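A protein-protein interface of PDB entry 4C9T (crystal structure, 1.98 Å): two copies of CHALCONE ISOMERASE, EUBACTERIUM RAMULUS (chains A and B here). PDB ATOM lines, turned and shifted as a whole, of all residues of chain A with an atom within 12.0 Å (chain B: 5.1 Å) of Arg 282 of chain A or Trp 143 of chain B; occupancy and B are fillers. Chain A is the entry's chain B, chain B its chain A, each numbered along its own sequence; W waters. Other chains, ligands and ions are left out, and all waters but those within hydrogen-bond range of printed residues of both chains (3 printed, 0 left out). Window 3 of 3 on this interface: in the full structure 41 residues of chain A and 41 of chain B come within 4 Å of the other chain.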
ATOM      1  N   TYR A 278       4.245  18.928  13.961  1.00  0.00           N
ATOM      2  CA  TYR A 278       2.925  19.465  14.367  1.00  0.00           C
ATOM      3  C   TYR A 278       2.615  18.940  15.766  1.00  0.00           C
ATOM      4  O   TYR A 278       1.933  17.945  15.956  1.00  0.00           O
ATOM      5  CB  TYR A 278       1.878  19.080  13.327  1.00  0.00           C
ATOM      6  CG  TYR A 278       0.573  19.790  13.483  1.00  0.00           C
ATOM      7  CD1 TYR A 278       0.368  21.073  12.987  1.00  0.00           C
ATOM      8  CD2 TYR A 278      -0.513  19.141  14.015  1.00  0.00           C
ATOM      9  CE1 TYR A 278      -0.859  21.695  13.066  1.00  0.00           C
ATOM     10  CE2 TYR A 278      -1.745  19.761  14.088  1.00  0.00           C
ATOM     11  CZ  TYR A 278      -1.897  21.011  13.624  1.00  0.00           C
ATOM     12  OH  TYR A 278      -3.105  21.590  13.745  1.00  0.00           O
ATOM     13  N   ILE A 279       3.153  19.625  16.745  1.00  0.00           N
ATOM     14  CA  ILE A 279       2.992  19.279  18.136  1.00  0.00           C
ATOM     15  C   ILE A 279       1.656  19.809  18.615  1.00  0.00           C
ATOM     16  O   ILE A 279       1.357  20.981  18.436  1.00  0.00           O
ATOM     17  CB  ILE A 279       4.176  19.859  18.968  1.00  0.00           C
ATOM     18  CG1 ILE A 279       5.532  19.303  18.475  1.00  0.00           C
ATOM     19  CG2 ILE A 279       4.009  19.592  20.447  1.00  0.00           C
ATOM     20  CD1 ILE A 279       5.616  17.811  18.193  1.00  0.00           C
ATOM     21  N   THR A 280       0.826  18.938  19.180  1.00  0.00           N
ATOM     22  CA  THR A 280      -0.494  19.335  19.550  1.00  0.00           C
ATOM     23  C   THR A 280      -0.608  19.674  21.060  1.00  0.00           C
ATOM     24  O   THR A 280       0.017  19.023  21.872  1.00  0.00           O
ATOM     25  CB  THR A 280      -1.542  18.260  19.217  1.00  0.00           C
ATOM     26  OG1 THR A 280      -1.207  16.991  19.799  1.00  0.00           O
ATOM     27  CG2 THR A 280      -1.630  18.143  17.700  1.00  0.00           C
ATOM     28  N   MET A 281      -1.479  20.611  21.380  1.00  0.00           N
ATOM     29  CA  MET A 281      -1.751  20.978  22.774  1.00  0.00           C
ATOM     30  C   MET A 281      -2.327  19.849  23.572  1.00  0.00           C
ATOM     31  O   MET A 281      -3.119  19.054  23.086  1.00  0.00           O
ATOM     32  CB  MET A 281      -2.672  22.171  22.830  1.00  0.00           C
ATOM     33  CG  MET A 281      -2.815  22.723  24.230  1.00  0.00           C
ATOM     34  SD  MET A 281      -3.947  24.409  24.172  1.00  0.00           S
ATOM     35  CE  MET A 281      -5.501  23.727  23.399  1.00  0.00           C
ATOM     36  N   ARG A 282      -1.915  19.812  24.821  1.00  0.00           N
ATOM     37  CA  ARG A 282      -2.341  18.793  25.793  1.00  0.00           C
ATOM     38  C   ARG A 282      -3.687  19.084  26.473  1.00  0.00           C
ATOM     39  O   ARG A 282      -4.452  19.950  26.021  1.00  0.00           O
ATOM     40  CB  ARG A 282      -1.221  18.578  26.871  1.00  0.00           C
ATOM     41  CG  ARG A 282       0.162  18.184  26.289  1.00  0.00           C
ATOM     42  CD  ARG A 282       1.301  18.121  27.338  1.00  0.00           C
ATOM     43  NE  ARG A 282       0.962  17.036  28.209  1.00  0.00           N
ATOM     44  CZ  ARG A 282       0.342  17.110  29.369  1.00  0.00           C
ATOM     45  NH1 ARG A 282       0.131  18.231  30.024  1.00  0.00           N
ATOM     46  NH2 ARG A 282      -0.030  15.990  29.918  1.00  0.00           N
ATOM     47  OXT ARG A 282      -4.050  18.435  27.497  1.00  0.00           O
ATOM     48  N   PRO B   7       4.621  18.847  39.872  1.00  0.00           N
ATOM     49  CA  PRO B   7       4.403  19.047  38.472  1.00  0.00           C
ATOM     50  C   PRO B   7       2.996  19.611  38.290  1.00  0.00           C
ATOM     51  O   PRO B   7       1.996  19.076  38.815  1.00  0.00           O
ATOM     52  CB  PRO B   7       4.559  17.618  37.865  1.00  0.00           C
ATOM     53  CG  PRO B   7       4.230  16.706  39.033  1.00  0.00           C
ATOM     54  CD  PRO B   7       4.754  17.402  40.216  1.00  0.00           C
ATOM     55  N   ARG B   9       0.423  22.186  35.427  1.00  0.00           N
ATOM     56  CA  ARG B   9       0.235  22.979  34.208  1.00  0.00           C
ATOM     57  C   ARG B   9      -0.567  24.203  34.632  1.00  0.00           C
ATOM     58  O   ARG B   9      -1.525  24.068  35.371  1.00  0.00           O
ATOM     59  CB  ARG B   9      -0.569  22.176  33.239  1.00  0.00           C
ATOM     60  CG  ARG B   9      -0.885  22.893  31.960  1.00  0.00           C
ATOM     61  CD  ARG B   9      -1.830  22.071  31.130  1.00  0.00           C
ATOM     62  NE  ARG B   9      -2.000  22.614  29.812  1.00  0.00           N
ATOM     63  CZ  ARG B   9      -3.148  22.651  29.129  1.00  0.00           C
ATOM     64  NH1 ARG B   9      -4.314  22.264  29.658  1.00  0.00           N
ATOM     65  NH2 ARG B   9      -3.143  23.144  27.908  1.00  0.00           N
ATOM     66  N   GLU B  72       0.651  29.254  28.646  1.00  0.00           N
ATOM     67  CA  GLU B  72       0.744  27.949  29.305  1.00  0.00           C
ATOM     68  C   GLU B  72       2.164  27.642  29.813  1.00  0.00           C
ATOM     69  O   GLU B  72       3.111  27.784  29.073  1.00  0.00           O
ATOM     70  CB  GLU B  72       0.389  26.897  28.253  1.00  0.00           C
ATOM     71  CG  GLU B  72       0.281  25.468  28.771  1.00  0.00           C
ATOM     72  CD  GLU B  72       0.429  24.470  27.631  1.00  0.00           C
ATOM     73  OE1 GLU B  72       1.372  24.572  26.787  1.00  0.00           O
ATOM     74  OE2 GLU B  72      -0.386  23.564  27.583  1.00  0.00           O
ATOM     75  N   HIS B  74       4.380  24.634  32.097  1.00  0.00           N
ATOM     76  CA  HIS B  74       4.462  23.388  32.860  1.00  0.00           C
ATOM     77  C   HIS B  74       5.610  23.498  33.839  1.00  0.00           C
ATOM     78  O   HIS B  74       6.769  23.628  33.425  1.00  0.00           O
ATOM     79  CB  HIS B  74       4.675  22.217  31.907  1.00  0.00           C
ATOM     80  CG  HIS B  74       3.455  21.838  31.102  1.00  0.00           C
ATOM     81  ND1 HIS B  74       3.068  22.530  29.977  1.00  0.00           N
ATOM     82  CD2 HIS B  74       2.603  20.749  31.198  1.00  0.00           C
ATOM     83  CE1 HIS B  74       1.979  21.975  29.456  1.00  0.00           C
ATOM     84  NE2 HIS B  74       1.692  20.859  30.165  1.00  0.00           N
ATOM     85  N   PRO B 141      -3.395  20.149  37.646  1.00  0.00           N
ATOM     86  CA  PRO B 141      -2.544  19.026  37.400  1.00  0.00           C
ATOM     87  C   PRO B 141      -2.152  18.963  35.925  1.00  0.00           C
ATOM     88  O   PRO B 141      -2.854  19.528  35.060  1.00  0.00           O
ATOM     89  CB  PRO B 141      -3.418  17.833  37.827  1.00  0.00           C
ATOM     90  CG  PRO B 141      -4.831  18.275  37.583  1.00  0.00           C
ATOM     91  CD  PRO B 141      -4.774  19.732  37.987  1.00  0.00           C
ATOM     92  N   MET B 142      -1.054  18.277  35.610  1.00  0.00           N
ATOM     93  CA  MET B 142      -0.620  18.154  34.212  1.00  0.00           C
ATOM     94  C   MET B 142      -1.546  17.381  33.341  1.00  0.00           C
ATOM     95  O   MET B 142      -1.463  17.449  32.097  1.00  0.00           O
ATOM     96  CB  MET B 142       0.768  17.608  34.101  1.00  0.00           C
ATOM     97  CG  MET B 142       1.847  18.556  34.609  1.00  0.00           C
ATOM     98  SD  MET B 142       3.625  17.783  34.016  1.00  0.00           S
ATOM     99  CE  MET B 142       4.823  19.308  34.559  1.00  0.00           C
ATOM    100  N   TRP B 143      -2.351  16.544  33.971  1.00  0.00           N
ATOM    101  CA  TRP B 143      -3.289  15.684  33.239  1.00  0.00           C
ATOM    102  C   TRP B 143      -4.722  16.006  33.618  1.00  0.00           C
ATOM    103  O   TRP B 143      -5.074  16.191  34.780  1.00  0.00           O
ATOM    104  CB  TRP B 143      -2.976  14.242  33.520  1.00  0.00           C
ATOM    105  CG  TRP B 143      -1.564  13.916  33.167  1.00  0.00           C
ATOM    106  CD1 TRP B 143      -1.062  13.513  31.911  1.00  0.00           C
ATOM    107  CD2 TRP B 143      -0.414  14.040  34.028  1.00  0.00           C
ATOM    108  NE1 TRP B 143       0.306  13.416  31.983  1.00  0.00           N
ATOM    109  CE2 TRP B 143       0.746  13.737  33.210  1.00  0.00           C
ATOM    110  CE3 TRP B 143      -0.231  14.399  35.352  1.00  0.00           C
ATOM    111  CZ2 TRP B 143       2.040  13.788  33.731  1.00  0.00           C
ATOM    112  CZ3 TRP B 143       1.035  14.453  35.863  1.00  0.00           C
ATOM    113  CH2 TRP B 143       2.150  14.142  35.077  1.00  0.00           C
ATOM    114  N   TRP B 144      -5.573  16.017  32.619  1.00  0.00           N
ATOM    115  CA  TRP B 144      -6.957  16.320  32.840  1.00  0.00           C
ATOM    116  C   TRP B 144      -7.558  15.317  33.800  1.00  0.00           C
ATOM    117  O   TRP B 144      -7.304  14.096  33.710  1.00  0.00           O
ATOM    118  CB  TRP B 144      -7.730  16.267  31.542  1.00  0.00           C
ATOM    119  CG  TRP B 144      -7.394  17.395  30.613  1.00  0.00           C
ATOM    120  CD1 TRP B 144      -6.597  17.367  29.495  1.00  0.00           C
ATOM    121  CD2 TRP B 144      -7.846  18.741  30.735  1.00  0.00           C
ATOM    122  NE1 TRP B 144      -6.529  18.591  28.910  1.00  0.00           N
ATOM    123  CE2 TRP B 144      -7.299  19.464  29.595  1.00  0.00           C
ATOM    124  CE3 TRP B 144      -8.705  19.392  31.612  1.00  0.00           C
ATOM    125  CZ2 TRP B 144      -7.579  20.786  29.363  1.00  0.00           C
ATOM    126  CZ3 TRP B 144      -8.971  20.744  31.377  1.00  0.00           C
ATOM    127  CH2 TRP B 144      -8.391  21.418  30.281  1.00  0.00           C
ATOM    128  N   GLU B 145      -8.345  15.803  34.722  1.00  0.00           N
ATOM    129  CA  GLU B 145      -8.939  14.904  35.752  1.00  0.00           C
ATOM    130  C   GLU B 145     -10.173  14.169  35.277  1.00  0.00           C
ATOM    131  O   GLU B 145     -10.379  13.067  35.731  1.00  0.00           O
ATOM    132  CB  GLU B 145      -9.270  15.637  37.043  1.00  0.00           C
ATOM    133  CG  GLU B 145      -8.046  16.257  37.662  1.00  0.00           C
ATOM    134  CD  GLU B 145      -8.308  17.107  38.887  1.00  0.00           C
ATOM    135  OE1 GLU B 145      -9.365  17.764  38.990  1.00  0.00           O
ATOM    136  OE2 GLU B 145      -7.401  17.131  39.743  1.00  0.00           O
ATOM    137  N   ARG B 162     -10.821  24.559  19.844  1.00  0.00           N
ATOM    138  CA  ARG B 162     -10.664  24.179  21.251  1.00  0.00           C
ATOM    139  C   ARG B 162     -11.032  25.322  22.156  1.00  0.00           C
ATOM    140  O   ARG B 162     -10.265  26.276  22.230  1.00  0.00           O
ATOM    141  CB  ARG B 162      -9.243  23.709  21.484  1.00  0.00           C
ATOM    142  CG  ARG B 162      -8.892  22.494  20.619  1.00  0.00           C
ATOM    143  CD  ARG B 162      -7.434  22.032  20.710  1.00  0.00           C
ATOM    144  NE  ARG B 162      -7.069  21.508  22.043  1.00  0.00           N
ATOM    145  CZ  ARG B 162      -6.120  20.632  22.289  1.00  0.00           C
ATOM    146  NH1 ARG B 162      -5.400  20.125  21.319  1.00  0.00           N
ATOM    147  NH2 ARG B 162      -5.909  20.310  23.535  1.00  0.00           N
ATOM    148  N   SER B 202     -10.721  19.794  34.743  1.00  0.00           N
ATOM    149  CA  SER B 202      -9.974  19.686  35.975  1.00  0.00           C
ATOM    150  C   SER B 202     -10.395  20.728  37.005  1.00  0.00           C
ATOM    151  O   SER B 202     -10.750  21.836  36.666  1.00  0.00           O
ATOM    152  CB  SER B 202      -8.455  19.819  35.755  1.00  0.00           C
ATOM    153  OG  SER B 202      -7.963  18.682  35.035  1.00  0.00           O
ATOM    154  N   GLU B 218     -12.230  22.231  28.895  1.00  0.00           N
ATOM    155  CA  GLU B 218     -11.924  22.452  27.519  1.00  0.00           C
ATOM    156  C   GLU B 218     -12.944  21.690  26.686  1.00  0.00           C
ATOM    157  O   GLU B 218     -13.214  20.539  26.946  1.00  0.00           O
ATOM    158  CB  GLU B 218     -10.515  22.051  27.193  1.00  0.00           C
ATOM    159  CG  GLU B 218     -10.082  22.638  25.872  1.00  0.00           C
ATOM    160  CD  GLU B 218      -8.602  22.495  25.568  1.00  0.00           C
ATOM    161  OE1 GLU B 218      -7.799  23.149  26.273  1.00  0.00           O
ATOM    162  OE2 GLU B 218      -8.232  21.705  24.636  1.00  0.00           O
HETATM  163  O   HOH W   1      -5.614  22.189  26.957  1.00  0.00           O
HETATM  164  O   HOH W   2      -3.301  18.751  30.160  1.00  0.00           O
HETATM  165  O   HOH W   3       0.050  21.436  25.914  1.00  0.00           O
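The chain-end carboxylate of Arg 282 of chain A is in salt-bridge range of the guanidinium group of Arg 9 of chain B, at 3.9 Å.
The guanidinium group of Arg 282 of chain A is in hydrogen-bond range of a ring nitrogen (NE2) of His 74 of chain B, at 3.1 Å.
The backbone carbonyl oxygen of Met 142 of chain B lies within hydrogen-bond range of the guanidinium group of Arg 282 of chain A, at 2.7 Å.
The indole nitrogen (NE1) of Trp 144 of chain B sits at hydrogen-bond distance from the chain-end carboxylate (OXT) of Arg 282 of chain A, 2.9 Å away.
NH1 of Arg 162 of chain B lies within hydrogen-bond range of O of Met 281 of chain A, 3.1 Å away.
The guanidinium group (NH2) of Arg 162 of chain B is in salt-bridge range of the chain-end carboxylate (O) of Arg 282 of chain A (2.9 Å).
The guanidinium group (NH2) of Arg 282 of chain A sits close to the indole nitrogen (NE1) of Trp 143 of chain B (3.3 Å).
Of the 12 printed residues of chain B, 7 touch a printed residue of chain A.
Hydrophobic or aromatic side chains of chain A within 4 Å of the printed part of chain B: Met 281.
Among the printed residues, 9 pairs touch across the chains.
No position is printed for both chains.
Of the 9 pairs that touch across the chains among the printed residues, none has its exchanged pair printed and touching as well.
Arg 9 of chain B touches Met 281 of chain A (NH2 to CG, 3.7 Å).
Met 281 of chain A touches Glu 218 of chain B.
Of chain B, only Arg 9 (3.9 Å), His 74 (3.1 Å), Met 142 (2.7 Å), Trp 143 (3.3 Å), Trp 144 (2.9 Å) and Arg 162 (2.9 Å) come within 4 Å of Arg 282 of chain A.
Of the printed residues of chain A, Trp 143 of chain B touches Arg 282.
Arg 9 of chain B touches two residues of chain A.
Of chain A, only Arg 282 (2.9 Å) comes within 4 Å of Trp 144 of chain B.
No residue of chain A comes within 4 Å of Glu 145 of chain B.
Printed residues of chain A within 4 Å of Glu 218 of chain B: Met 281 (3.6 Å).
Of the printed residues of chain A, His 74 of chain B touches Arg 282 (3.1 Å).
Of the printed residues of chain B, Met 281 of chain A touches Arg 9 (3.7 Å), Arg 162 (3.0 Å) and Glu 218 (3.6 Å).
Tyr 278 of chain A touches none of the printed residues of chain B.
The nearest residue of chain B that does not touch Arg 282 of chain A is Glu 218 of chain B (4.4 Å).
The nearest residue of chain A that does not touch Trp 143 of chain B is Met 281 of chain A (10.5 Å).
OE2 of Glu 72 of chain B is in salt-bridge range of NH2 of Arg 9 of chain B (2.8 Å).
The guanidinium group (NE) of Arg 162 of chain B is in salt-bridge range of the side-chain carboxylate (OE2) of Glu 218 of chain B, 2.8 Å away.
Water W1 lies within hydrogen-bond range of the side-chain carboxylate of Glu 218 of chain B, the chain-end carboxylate of Arg 282 of chain A and the guanidinium group of Arg 9 of chain B.
Water W3 bridges OE2 of Glu 72 of chain B and N of Arg 282 of chain A.
Water W2 lies within hydrogen-bond range of the chain-end carboxylate of Arg 282 of chain A (2.8 Å), the backbone carbonyl oxygen of Met 142 of chain B (3.0 Å) and the indole nitrogen of Trp 144 of chain B (3.5 Å).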
